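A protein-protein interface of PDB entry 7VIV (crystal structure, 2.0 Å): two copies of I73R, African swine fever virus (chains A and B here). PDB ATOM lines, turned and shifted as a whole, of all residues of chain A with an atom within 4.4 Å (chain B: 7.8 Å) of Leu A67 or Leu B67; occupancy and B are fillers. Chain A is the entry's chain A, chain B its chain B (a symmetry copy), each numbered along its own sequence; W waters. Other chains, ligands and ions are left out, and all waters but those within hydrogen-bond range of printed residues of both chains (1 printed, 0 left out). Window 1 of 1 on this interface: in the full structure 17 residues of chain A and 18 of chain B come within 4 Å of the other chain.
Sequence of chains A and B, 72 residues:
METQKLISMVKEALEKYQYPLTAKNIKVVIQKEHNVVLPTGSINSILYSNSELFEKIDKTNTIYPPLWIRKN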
ATOM      1  N   TYR A  19     -24.509  19.518  10.822  1.00  0.00           N
ATOM      2  CA  TYR A  19     -25.135  20.595  11.577  1.00  0.00           C
ATOM      3  C   TYR A  19     -25.722  21.612  10.619  1.00  0.00           C
ATOM      4  O   TYR A  19     -25.414  21.560   9.421  1.00  0.00           O
ATOM      5  CB  TYR A  19     -24.151  21.215  12.576  1.00  0.00           C
ATOM      6  CG  TYR A  19     -22.755  21.489  12.065  1.00  0.00           C
ATOM      7  CD1 TYR A  19     -21.741  20.573  12.319  1.00  0.00           C
ATOM      8  CD2 TYR A  19     -22.453  22.603  11.294  1.00  0.00           C
ATOM      9  CE1 TYR A  19     -20.446  20.773  11.880  1.00  0.00           C
ATOM     10  CE2 TYR A  19     -21.143  22.815  10.825  1.00  0.00           C
ATOM     11  CZ  TYR A  19     -20.144  21.890  11.128  1.00  0.00           C
ATOM     12  OH  TYR A  19     -18.839  22.063  10.684  1.00  0.00           O
ATOM     13  N   PRO A  20     -26.620  22.493  11.070  1.00  0.00           N
ATOM     14  CA  PRO A  20     -27.223  23.454  10.144  1.00  0.00           C
ATOM     15  C   PRO A  20     -26.180  24.448   9.638  1.00  0.00           C
ATOM     16  O   PRO A  20     -25.182  24.716  10.308  1.00  0.00           O
ATOM     17  CB  PRO A  20     -28.292  24.145  10.997  1.00  0.00           C
ATOM     18  CG  PRO A  20     -28.614  23.119  12.072  1.00  0.00           C
ATOM     19  CD  PRO A  20     -27.278  22.540  12.393  1.00  0.00           C
ATOM     20  N   LEU A  21     -26.436  25.002   8.444  1.00  0.00           N
ATOM     21  CA  LEU A  21     -25.528  25.904   7.749  1.00  0.00           C
ATOM     22  C   LEU A  21     -26.303  27.116   7.279  1.00  0.00           C
ATOM     23  O   LEU A  21     -27.466  26.992   6.910  1.00  0.00           O
ATOM     24  CB  LEU A  21     -24.896  25.225   6.519  1.00  0.00           C
ATOM     25  CG  LEU A  21     -24.111  23.942   6.768  1.00  0.00           C
ATOM     26  CD1 LEU A  21     -23.563  23.429   5.456  1.00  0.00           C
ATOM     27  CD2 LEU A  21     -22.981  24.231   7.771  1.00  0.00           C
ATOM     28  N   THR A  22     -25.655  28.281   7.257  1.00  0.00           N
ATOM     29  CA  THR A  22     -26.295  29.435   6.627  1.00  0.00           C
ATOM     30  C   THR A  22     -26.150  29.355   5.107  1.00  0.00           C
ATOM     31  O   THR A  22     -25.360  28.575   4.565  1.00  0.00           O
ATOM     32  CB  THR A  22     -25.678  30.753   7.097  1.00  0.00           C
ATOM     33  OG1 THR A  22     -24.316  30.798   6.667  1.00  0.00           O
ATOM     34  CG2 THR A  22     -25.678  30.831   8.590  1.00  0.00           C
ATOM     35  N   ASN A  25     -22.641  30.010   4.424  1.00  0.00           N
ATOM     36  CA  ASN A  25     -21.819  28.818   4.665  1.00  0.00           C
ATOM     37  C   ASN A  25     -21.889  27.878   3.474  1.00  0.00           C
ATOM     38  O   ASN A  25     -20.878  27.310   3.048  1.00  0.00           O
ATOM     39  CB  ASN A  25     -22.278  28.044   5.908  1.00  0.00           C
ATOM     40  CG  ASN A  25     -22.102  28.815   7.230  1.00  0.00           C
ATOM     41  OD1 ASN A  25     -22.814  28.531   8.183  1.00  0.00           O
ATOM     42  ND2 ASN A  25     -21.153  29.753   7.295  1.00  0.00           N
ATOM     43  N   LYS A  56     -35.689  25.624   7.458  1.00  0.00           N
ATOM     44  CA  LYS A  56     -34.930  26.285   8.515  1.00  0.00           C
ATOM     45  C   LYS A  56     -35.016  25.477   9.805  1.00  0.00           C
ATOM     46  O   LYS A  56     -36.091  25.004  10.184  1.00  0.00           O
ATOM     47  CB  LYS A  56     -35.461  27.696   8.757  1.00  0.00           C
ATOM     48  CG  LYS A  56     -35.275  28.675   7.605  1.00  0.00           C
ATOM     49  CD  LYS A  56     -36.052  29.963   7.913  1.00  0.00           C
ATOM     50  CE  LYS A  56     -36.117  30.890   6.716  1.00  0.00           C
ATOM     51  NZ  LYS A  56     -36.922  32.131   6.987  1.00  0.00           N
ATOM     52  N   ILE A  57     -33.873  25.294  10.474  1.00  0.00           N
ATOM     53  CA  ILE A  57     -33.894  24.579  11.754  1.00  0.00           C
ATOM     54  C   ILE A  57     -34.601  25.422  12.813  1.00  0.00           C
ATOM     55  O   ILE A  57     -35.187  24.878  13.755  1.00  0.00           O
ATOM     56  CB  ILE A  57     -32.468  24.175  12.201  1.00  0.00           C
ATOM     57  CG1 ILE A  57     -32.468  23.439  13.548  1.00  0.00           C
ATOM     58  CG2 ILE A  57     -31.582  25.394  12.386  1.00  0.00           C
ATOM     59  CD1 ILE A  57     -33.333  22.185  13.599  1.00  0.00           C
ATOM     60  N   ILE A  63     -33.327  33.216  14.551  1.00  0.00           N
ATOM     61  CA  ILE A  63     -31.977  33.035  14.012  1.00  0.00           C
ATOM     62  C   ILE A  63     -31.900  33.676  12.626  1.00  0.00           C
ATOM     63  O   ILE A  63     -32.529  33.204  11.676  1.00  0.00           O
ATOM     64  CB  ILE A  63     -31.585  31.558  13.955  1.00  0.00           C
ATOM     65  CG1 ILE A  63     -31.671  30.918  15.350  1.00  0.00           C
ATOM     66  CG2 ILE A  63     -30.177  31.419  13.422  1.00  0.00           C
ATOM     67  CD1 ILE A  63     -30.890  31.659  16.395  1.00  0.00           C
ATOM     68  N   PRO A  65     -28.752  35.511   9.966  1.00  0.00           N
ATOM     69  CA  PRO A  65     -29.272  34.815   8.772  1.00  0.00           C
ATOM     70  C   PRO A  65     -29.655  33.378   9.098  1.00  0.00           C
ATOM     71  O   PRO A  65     -28.993  32.764   9.926  1.00  0.00           O
ATOM     72  CB  PRO A  65     -28.092  34.857   7.789  1.00  0.00           C
ATOM     73  CG  PRO A  65     -26.912  35.102   8.628  1.00  0.00           C
ATOM     74  CD  PRO A  65     -27.376  35.978   9.747  1.00  0.00           C
ATOM     75  N   PRO A  66     -30.713  32.859   8.483  1.00  0.00           N
ATOM     76  CA  PRO A  66     -31.252  31.577   8.940  1.00  0.00           C
ATOM     77  C   PRO A  66     -30.257  30.444   8.755  1.00  0.00           C
ATOM     78  O   PRO A  66     -29.395  30.473   7.874  1.00  0.00           O
ATOM     79  CB  PRO A  66     -32.494  31.378   8.068  1.00  0.00           C
ATOM     80  CG  PRO A  66     -32.898  32.779   7.684  1.00  0.00           C
ATOM     81  CD  PRO A  66     -31.597  33.519   7.510  1.00  0.00           C
ATOM     82  N   LEU A  67     -30.388  29.454   9.622  1.00  0.00           N
ATOM     83  CA  LEU A  67     -29.625  28.219   9.567  1.00  0.00           C
ATOM     84  C   LEU A  67     -30.517  27.159   8.941  1.00  0.00           C
ATOM     85  O   LEU A  67     -31.689  27.050   9.305  1.00  0.00           O
ATOM     86  CB  LEU A  67     -29.189  27.778  10.966  1.00  0.00           C
ATOM     87  CG  LEU A  67     -28.041  28.570  11.623  1.00  0.00           C
ATOM     88  CD1 LEU A  67     -27.951  28.138  13.060  1.00  0.00           C
ATOM     89  CD2 LEU A  67     -26.695  28.334  10.912  1.00  0.00           C
ATOM     90  N   TRP A  68     -29.955  26.374   8.020  1.00  0.00           N
ATOM     91  CA  TRP A  68     -30.729  25.480   7.168  1.00  0.00           C
ATOM     92  C   TRP A  68     -30.273  24.042   7.330  1.00  0.00           C
ATOM     93  O   TRP A  68     -29.073  23.762   7.478  1.00  0.00           O
ATOM     94  CB  TRP A  68     -30.582  25.862   5.685  1.00  0.00           C
ATOM     95  CG  TRP A  68     -31.160  27.210   5.325  1.00  0.00           C
ATOM     96  CD1 TRP A  68     -30.528  28.430   5.371  1.00  0.00           C
ATOM     97  CD2 TRP A  68     -32.487  27.460   4.857  1.00  0.00           C
ATOM     98  NE1 TRP A  68     -31.400  29.425   4.949  1.00  0.00           N
ATOM     99  CE2 TRP A  68     -32.598  28.843   4.618  1.00  0.00           C
ATOM    100  CE3 TRP A  68     -33.591  26.639   4.602  1.00  0.00           C
ATOM    101  CZ2 TRP A  68     -33.766  29.415   4.155  1.00  0.00           C
ATOM    102  CZ3 TRP A  68     -34.735  27.214   4.140  1.00  0.00           C
ATOM    103  CH2 TRP A  68     -34.819  28.583   3.923  1.00  0.00           C
ATOM    104  N   LEU B  14     -25.796  31.126  22.871  1.00  0.00           N
ATOM    105  CA  LEU B  14     -25.393  29.791  22.453  1.00  0.00           C
ATOM    106  C   LEU B  14     -26.163  28.733  23.218  1.00  0.00           C
ATOM    107  O   LEU B  14     -26.629  27.751  22.630  1.00  0.00           O
ATOM    108  CB  LEU B  14     -23.895  29.612  22.658  1.00  0.00           C
ATOM    109  CG  LEU B  14     -23.077  30.229  21.519  1.00  0.00           C
ATOM    110  CD1 LEU B  14     -21.622  30.352  21.920  1.00  0.00           C
ATOM    111  CD2 LEU B  14     -23.222  29.426  20.208  1.00  0.00           C
ATOM    112  N   TYR B  17     -29.695  27.474  22.159  1.00  0.00           N
ATOM    113  CA  TYR B  17     -29.879  26.689  20.943  1.00  0.00           C
ATOM    114  C   TYR B  17     -29.021  25.424  20.974  1.00  0.00           C
ATOM    115  O   TYR B  17     -27.953  25.393  21.590  1.00  0.00           O
ATOM    116  CB  TYR B  17     -29.582  27.564  19.713  1.00  0.00           C
ATOM    117  CG  TYR B  17     -30.601  28.676  19.587  1.00  0.00           C
ATOM    118  CD1 TYR B  17     -31.785  28.468  18.899  1.00  0.00           C
ATOM    119  CD2 TYR B  17     -30.410  29.908  20.204  1.00  0.00           C
ATOM    120  CE1 TYR B  17     -32.733  29.446  18.804  1.00  0.00           C
ATOM    121  CE2 TYR B  17     -31.362  30.904  20.120  1.00  0.00           C
ATOM    122  CZ  TYR B  17     -32.528  30.662  19.411  1.00  0.00           C
ATOM    123  OH  TYR B  17     -33.516  31.617  19.296  1.00  0.00           O
ATOM    124  N   TYR B  19     -27.511  23.868  18.493  1.00  0.00           N
ATOM    125  CA  TYR B  19     -26.673  23.750  17.312  1.00  0.00           C
ATOM    126  C   TYR B  19     -25.757  24.961  17.236  1.00  0.00           C
ATOM    127  O   TYR B  19     -26.023  25.979  17.881  1.00  0.00           O
ATOM    128  CB  TYR B  19     -27.533  23.646  16.044  1.00  0.00           C
ATOM    129  CG  TYR B  19     -28.739  24.543  16.043  1.00  0.00           C
ATOM    130  CD1 TYR B  19     -29.981  24.066  16.445  1.00  0.00           C
ATOM    131  CD2 TYR B  19     -28.649  25.857  15.619  1.00  0.00           C
ATOM    132  CE1 TYR B  19     -31.103  24.891  16.435  1.00  0.00           C
ATOM    133  CE2 TYR B  19     -29.757  26.682  15.607  1.00  0.00           C
ATOM    134  CZ  TYR B  19     -30.986  26.193  16.013  1.00  0.00           C
ATOM    135  OH  TYR B  19     -32.096  27.017  15.999  1.00  0.00           O
ATOM    136  N   PRO B  20     -24.674  24.883  16.452  1.00  0.00           N
ATOM    137  CA  PRO B  20     -23.742  26.009  16.371  1.00  0.00           C
ATOM    138  C   PRO B  20     -24.387  27.230  15.735  1.00  0.00           C
ATOM    139  O   PRO B  20     -25.256  27.117  14.866  1.00  0.00           O
ATOM    140  CB  PRO B  20     -22.610  25.465  15.492  1.00  0.00           C
ATOM    141  CG  PRO B  20     -22.752  23.991  15.554  1.00  0.00           C
ATOM    142  CD  PRO B  20     -24.211  23.750  15.635  1.00  0.00           C
ATOM    143  N   LEU B  21     -23.929  28.408  16.167  1.00  0.00           N
ATOM    144  CA  LEU B  21     -24.405  29.688  15.668  1.00  0.00           C
ATOM    145  C   LEU B  21     -23.240  30.498  15.132  1.00  0.00           C
ATOM    146  O   LEU B  21     -22.101  30.355  15.597  1.00  0.00           O
ATOM    147  CB  LEU B  21     -25.077  30.503  16.767  1.00  0.00           C
ATOM    148  CG  LEU B  21     -26.258  29.913  17.516  1.00  0.00           C
ATOM    149  CD1 LEU B  21     -26.724  30.890  18.599  1.00  0.00           C
ATOM    150  CD2 LEU B  21     -27.384  29.579  16.540  1.00  0.00           C
ATOM    151  N   THR B  22     -23.530  31.371  14.165  1.00  0.00           N
ATOM    152  CA  THR B  22     -22.515  32.335  13.760  1.00  0.00           C
ATOM    153  C   THR B  22     -22.487  33.494  14.742  1.00  0.00           C
ATOM    154  O   THR B  22     -23.366  33.631  15.596  1.00  0.00           O
ATOM    155  CB  THR B  22     -22.773  32.891  12.362  1.00  0.00           C
ATOM    156  OG1 THR B  22     -23.872  33.805  12.436  1.00  0.00           O
ATOM    157  CG2 THR B  22     -23.077  31.768  11.353  1.00  0.00           C
ATOM    158  N   ALA B  23     -21.450  34.332  14.609  1.00  0.00           N
ATOM    159  CA  ALA B  23     -21.341  35.532  15.442  1.00  0.00           C
ATOM    160  C   ALA B  23     -22.513  36.470  15.189  1.00  0.00           C
ATOM    161  O   ALA B  23     -23.020  37.130  16.107  1.00  0.00           O
ATOM    162  CB  ALA B  23     -20.018  36.252  15.149  1.00  0.00           C
ATOM    163  N   ASN B  25     -25.531  35.504  14.077  1.00  0.00           N
ATOM    164  CA  ASN B  25     -26.687  34.885  14.727  1.00  0.00           C
ATOM    165  C   ASN B  25     -26.792  35.329  16.173  1.00  0.00           C
ATOM    166  O   ASN B  25     -27.880  35.671  16.667  1.00  0.00           O
ATOM    167  CB  ASN B  25     -26.581  33.355  14.702  1.00  0.00           C
ATOM    168  CG  ASN B  25     -26.691  32.768  13.316  1.00  0.00           C
ATOM    169  OD1 ASN B  25     -26.164  31.696  13.069  1.00  0.00           O
ATOM    170  ND2 ASN B  25     -27.388  33.451  12.413  1.00  0.00           N
ATOM    171  N   ILE B  26     -25.670  35.255  16.885  1.00  0.00           N
ATOM    172  CA  ILE B  26     -25.648  35.624  18.294  1.00  0.00           C
ATOM    173  C   ILE B  26     -26.059  37.080  18.453  1.00  0.00           C
ATOM    174  O   ILE B  26     -26.873  37.422  19.325  1.00  0.00           O
ATOM    175  CB  ILE B  26     -24.250  35.326  18.872  1.00  0.00           C
ATOM    176  CG1 ILE B  26     -23.981  33.820  18.796  1.00  0.00           C
ATOM    177  CG2 ILE B  26     -24.114  35.810  20.294  1.00  0.00           C
ATOM    178  CD1 ILE B  26     -22.514  33.433  18.982  1.00  0.00           C
ATOM    179  N   LEU B  47     -15.849  36.199  21.328  1.00  0.00           N
ATOM    180  CA  LEU B  47     -15.723  34.776  21.000  1.00  0.00           C
ATOM    181  C   LEU B  47     -14.262  34.344  20.915  1.00  0.00           C
ATOM    182  O   LEU B  47     -13.893  33.265  21.396  1.00  0.00           O
ATOM    183  CB  LEU B  47     -16.436  34.471  19.677  1.00  0.00           C
ATOM    184  CG  LEU B  47     -17.963  34.571  19.659  1.00  0.00           C
ATOM    185  CD1 LEU B  47     -18.430  34.616  18.215  1.00  0.00           C
ATOM    186  CD2 LEU B  47     -18.629  33.406  20.427  1.00  0.00           C
ATOM    187  N   GLU B  55     -15.671  27.839  21.210  1.00  0.00           N
ATOM    188  CA  GLU B  55     -14.808  27.301  20.168  1.00  0.00           C
ATOM    189  C   GLU B  55     -15.595  27.158  18.870  1.00  0.00           C
ATOM    190  O   GLU B  55     -16.821  27.042  18.883  1.00  0.00           O
ATOM    191  CB  GLU B  55     -14.214  25.945  20.559  1.00  0.00           C
ATOM    192  CG  GLU B  55     -15.194  24.796  20.542  1.00  0.00           C
ATOM    193  CD  GLU B  55     -14.476  23.466  20.403  1.00  0.00           C
ATOM    194  OE1 GLU B  55     -13.721  23.332  19.419  1.00  0.00           O
ATOM    195  OE2 GLU B  55     -14.643  22.573  21.267  1.00  0.00           O
ATOM    196  N   LYS B  56     -14.877  27.161  17.745  1.00  0.00           N
ATOM    197  CA  LYS B  56     -15.497  26.911  16.449  1.00  0.00           C
ATOM    198  C   LYS B  56     -15.704  25.419  16.274  1.00  0.00           C
ATOM    199  O   LYS B  56     -14.875  24.616  16.700  1.00  0.00           O
ATOM    200  CB  LYS B  56     -14.620  27.421  15.319  1.00  0.00           C
ATOM    201  CG  LYS B  56     -14.414  28.900  15.299  1.00  0.00           C
ATOM    202  CD  LYS B  56     -13.661  29.265  14.022  1.00  0.00           C
ATOM    203  CE  LYS B  56     -12.397  30.054  14.316  1.00  0.00           C
ATOM    204  NZ  LYS B  56     -11.915  30.703  13.052  1.00  0.00           N
ATOM    205  N   ILE B  57     -16.800  25.039  15.628  1.00  0.00           N
ATOM    206  CA  ILE B  57     -17.039  23.610  15.468  1.00  0.00           C
ATOM    207  C   ILE B  57     -16.322  23.049  14.240  1.00  0.00           C
ATOM    208  O   ILE B  57     -15.936  21.876  14.229  1.00  0.00           O
ATOM    209  CB  ILE B  57     -18.548  23.314  15.435  1.00  0.00           C
ATOM    210  CG1 ILE B  57     -18.798  21.802  15.505  1.00  0.00           C
ATOM    211  CG2 ILE B  57     -19.197  23.931  14.209  1.00  0.00           C
ATOM    212  CD1 ILE B  57     -20.221  21.416  15.804  1.00  0.00           C
ATOM    213  N   ASP B  58     -16.127  23.839  13.196  1.00  0.00           N
ATOM    214  CA  ASP B  58     -15.339  23.403  12.047  1.00  0.00           C
ATOM    215  C   ASP B  58     -13.881  23.791  12.193  1.00  0.00           C
ATOM    216  O   ASP B  58     -13.559  24.969  12.369  1.00  0.00           O
ATOM    217  CB  ASP B  58     -15.882  23.950  10.730  1.00  0.00           C
ATOM    218  CG  ASP B  58     -14.931  23.689   9.556  1.00  0.00           C
ATOM    219  OD1 ASP B  58     -14.701  22.516   9.190  1.00  0.00           O
ATOM    220  OD2 ASP B  58     -14.458  24.696   8.967  1.00  0.00           O
ATOM    221  N   LYS B  59     -13.005  22.795  12.075  1.00  0.00           N
ATOM    222  CA  LYS B  59     -11.568  22.987  12.219  1.00  0.00           C
ATOM    223  C   LYS B  59     -10.820  22.686  10.925  1.00  0.00           C
ATOM    224  O   LYS B  59      -9.615  22.419  10.954  1.00  0.00           O
ATOM    225  CB  LYS B  59     -11.048  22.124  13.367  1.00  0.00           C
ATOM    226  CG  LYS B  59     -11.240  22.800  14.711  1.00  0.00           C
ATOM    227  CD  LYS B  59     -11.544  21.805  15.798  1.00  0.00           C
ATOM    228  CE  LYS B  59     -12.271  22.501  16.926  1.00  0.00           C
ATOM    229  NZ  LYS B  59     -11.554  23.749  17.376  1.00  0.00           N
ATOM    230  N   ILE B  63     -15.914  26.323   6.870  1.00  0.00           N
ATOM    231  CA  ILE B  63     -17.152  27.017   7.220  1.00  0.00           C
ATOM    232  C   ILE B  63     -16.845  28.482   7.514  1.00  0.00           C
ATOM    233  O   ILE B  63     -16.203  28.798   8.519  1.00  0.00           O
ATOM    234  CB  ILE B  63     -17.838  26.366   8.422  1.00  0.00           C
ATOM    235  CG1 ILE B  63     -18.080  24.881   8.154  1.00  0.00           C
ATOM    236  CG2 ILE B  63     -19.147  27.100   8.711  1.00  0.00           C
ATOM    237  CD1 ILE B  63     -18.875  24.657   6.907  1.00  0.00           C
ATOM    238  N   TYR B  64     -17.331  29.379   6.658  1.00  0.00           N
ATOM    239  CA  TYR B  64     -17.260  30.806   6.914  1.00  0.00           C
ATOM    240  C   TYR B  64     -18.595  31.415   6.515  1.00  0.00           C
ATOM    241  O   TYR B  64     -19.159  31.043   5.476  1.00  0.00           O
ATOM    242  CB  TYR B  64     -16.127  31.497   6.132  1.00  0.00           C
ATOM    243  CG  TYR B  64     -14.752  30.938   6.432  1.00  0.00           C
ATOM    244  CD1 TYR B  64     -14.120  30.089   5.533  1.00  0.00           C
ATOM    245  CD2 TYR B  64     -14.077  31.287   7.601  1.00  0.00           C
ATOM    246  CE1 TYR B  64     -12.871  29.579   5.791  1.00  0.00           C
ATOM    247  CE2 TYR B  64     -12.831  30.785   7.874  1.00  0.00           C
ATOM    248  CZ  TYR B  64     -12.229  29.931   6.966  1.00  0.00           C
ATOM    249  OH  TYR B  64     -10.979  29.444   7.226  1.00  0.00           O
ATOM    250  N   PRO B  65     -19.114  32.364   7.295  1.00  0.00           N
ATOM    251  CA  PRO B  65     -18.532  32.775   8.572  1.00  0.00           C
ATOM    252  C   PRO B  65     -18.620  31.640   9.592  1.00  0.00           C
ATOM    253  O   PRO B  65     -19.544  30.817   9.511  1.00  0.00           O
ATOM    254  CB  PRO B  65     -19.389  33.981   8.976  1.00  0.00           C
ATOM    255  CG  PRO B  65     -20.647  33.826   8.200  1.00  0.00           C
ATOM    256  CD  PRO B  65     -20.235  33.231   6.899  1.00  0.00           C
ATOM    257  N   PRO B  66     -17.629  31.564  10.474  1.00  0.00           N
ATOM    258  CA  PRO B  66     -17.506  30.407  11.350  1.00  0.00           C
ATOM    259  C   PRO B  66     -18.759  30.169  12.182  1.00  0.00           C
ATOM    260  O   PRO B  66     -19.436  31.105  12.605  1.00  0.00           O
ATOM    261  CB  PRO B  66     -16.310  30.772  12.236  1.00  0.00           C
ATOM    262  CG  PRO B  66     -15.459  31.661  11.355  1.00  0.00           C
ATOM    263  CD  PRO B  66     -16.489  32.495  10.625  1.00  0.00           C
ATOM    264  N   LEU B  67     -19.039  28.893  12.422  1.00  0.00           N
ATOM    265  CA  LEU B  67     -20.083  28.451  13.338  1.00  0.00           C
ATOM    266  C   LEU B  67     -19.451  28.138  14.693  1.00  0.00           C
ATOM    267  O   LEU B  67     -18.459  27.398  14.760  1.00  0.00           O
ATOM    268  CB  LEU B  67     -20.775  27.206  12.777  1.00  0.00           C
ATOM    269  CG  LEU B  67     -21.777  27.469  11.651  1.00  0.00           C
ATOM    270  CD1 LEU B  67     -22.178  26.144  10.982  1.00  0.00           C
ATOM    271  CD2 LEU B  67     -23.006  28.222  12.172  1.00  0.00           C
ATOM    272  N   TRP B  68     -20.037  28.676  15.763  1.00  0.00           N
ATOM    273  CA  TRP B  68     -19.482  28.609  17.107  1.00  0.00           C
ATOM    274  C   TRP B  68     -20.362  27.783  18.031  1.00  0.00           C
ATOM    275  O   TRP B  68     -21.590  27.807  17.932  1.00  0.00           O
ATOM    276  CB  TRP B  68     -19.353  29.991  17.730  1.00  0.00           C
ATOM    277  CG  TRP B  68     -18.361  30.840  17.043  1.00  0.00           C
ATOM    278  CD1 TRP B  68     -18.552  31.581  15.913  1.00  0.00           C
ATOM    279  CD2 TRP B  68     -17.011  31.042  17.442  1.00  0.00           C
ATOM    280  NE1 TRP B  68     -17.380  32.239  15.576  1.00  0.00           N
ATOM    281  CE2 TRP B  68     -16.422  31.921  16.505  1.00  0.00           C
ATOM    282  CE3 TRP B  68     -16.232  30.551  18.496  1.00  0.00           C
ATOM    283  CZ2 TRP B  68     -15.103  32.334  16.604  1.00  0.00           C
ATOM    284  CZ3 TRP B  68     -14.910  30.958  18.587  1.00  0.00           C
ATOM    285  CH2 TRP B  68     -14.360  31.840  17.643  1.00  0.00           C
ATOM    286  N   ILE B  69     -19.717  27.096  18.972  1.00  0.00           N
ATOM    287  CA  ILE B  69     -20.404  26.345  20.015  1.00  0.00           C
ATOM    288  C   ILE B  69     -19.874  26.783  21.373  1.00  0.00           C
ATOM    289  O   ILE B  69     -18.724  27.209  21.519  1.00  0.00           O
ATOM    290  CB  ILE B  69     -20.254  24.804  19.859  1.00  0.00           C
ATOM    291  CG1 ILE B  69     -18.782  24.378  19.977  1.00  0.00           C
ATOM    292  CG2 ILE B  69     -20.874  24.309  18.560  1.00  0.00           C
ATOM    293  CD1 ILE B  69     -18.568  22.871  20.059  1.00  0.00           C
HETATM  294  O   HOH W   1     -25.445  24.928  13.044  1.00  0.00           O
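The backbone NH of Thr B22 lies within hydrogen-bond range of the side-chain amide oxygen of Asn B25, at 2.9 Å. The backbone NH of Ile A57 is in hydrogen-bond range of the backbone carbonyl oxygen of Leu A67. The side-chain carboxylate (OD2) of Asp B58 sits at hydrogen-bond distance from the backbone NH (N) of Ile B63 (3.0 Å). O of Leu A21 lies within hydrogen-bond range of N of Trp A68 (2.8 Å). OG1 of Thr A22 sits at hydrogen-bond distance from N of Asn A25, at 2.9 Å. O of Leu B21 is in hydrogen-bond range of N of Trp B68 (2.7 Å).
Water W1 bridges the backbone carbonyl oxygen (O) of Pro A20 (2.8 Å) and the backbone carbonyl oxygen (O) of Pro B20 (2.9 Å).
Ile B57 touches Tyr A19 (CG2 to CZ, 3.8 Å). Ile B63 touches Tyr A19. Tyr A19 touches Leu B67 (CE2 to CD1, 3.5 Å). Tyr B19 touches Pro A20 (CB to CD, 3.8 Å). Pro A20 touches Leu B67. Tyr B19 touches Ile A63 (OH to CG1, 3.98 Å). CG2 of Ile A63 touches ND2 of Asn B25 (3.6 Å). Leu A67 touches Tyr B19. Leu A67 touches Pro B20. Leu B67 touches Leu A67 (CD2 to CD2, 3.9 Å).
Pro A20 touches Leu B67, and with the chains exchanged Leu A67 touches Pro B20. Asn A25 touches Pro B65, and with the chains exchanged Pro A65 touches Asn B25. Asn A25 touches Leu B67, and with the chains exchanged Leu A67 touches Asn B25. Leu B67 touches its own counterpart, Leu A67. 12 positions are printed for both chains. Of the 23 pairs that touch across the chains among the printed residues, 20 have their exchanged pair printed and touching as well.
Hydrophobic or aromatic side chains of chain A within 4 Å of the printed part of chain B: Tyr A19, Pro A20, Leu A21, Ile A57, Ile A63, Pro A65 and Leu A67. Printed residues of chain B that touch a printed residue of chain A: Tyr B17, Tyr B19, Pro B20, Leu B21, Thr B22, Asn B25, Ile B57, Asp B58, Ile B63, Tyr B64, Pro B65 and Leu B67. Among the printed residues, 23 pairs touch across the chains. Among the printed residues, no Asp or Glu carboxylate lies within 4 Å of a Lys or Arg side-chain nitrogen of the other chain.
Printed residues of chain B within 4 Å of Pro A20: Tyr B19 and Leu B67. Of the printed residues of chain B, Asn A25 touches Ile B63, Tyr B64, Pro B65 and Leu B67. Leu A67 touches five residues of chain B. Of the printed residues of chain A, Ile B63 touches Tyr A19 and Asn A25. Of the printed residues of chain A, Tyr B64 touches Asn A25. Leu B67 touches five residues of chain A.
The side-chain amide nitrogen (ND2) of Asn A25 sits at hydrogen-bond distance from the backbone carbonyl oxygen (O) of Tyr B64 (3.0 Å). O of Pro B65 is in hydrogen-bond range of ND2 of Asn A25 (2.9 Å). The backbone carbonyl oxygen (O) of Pro A65 is in hydrogen-bond range of the side-chain amide nitrogen (ND2) of Asn B25.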
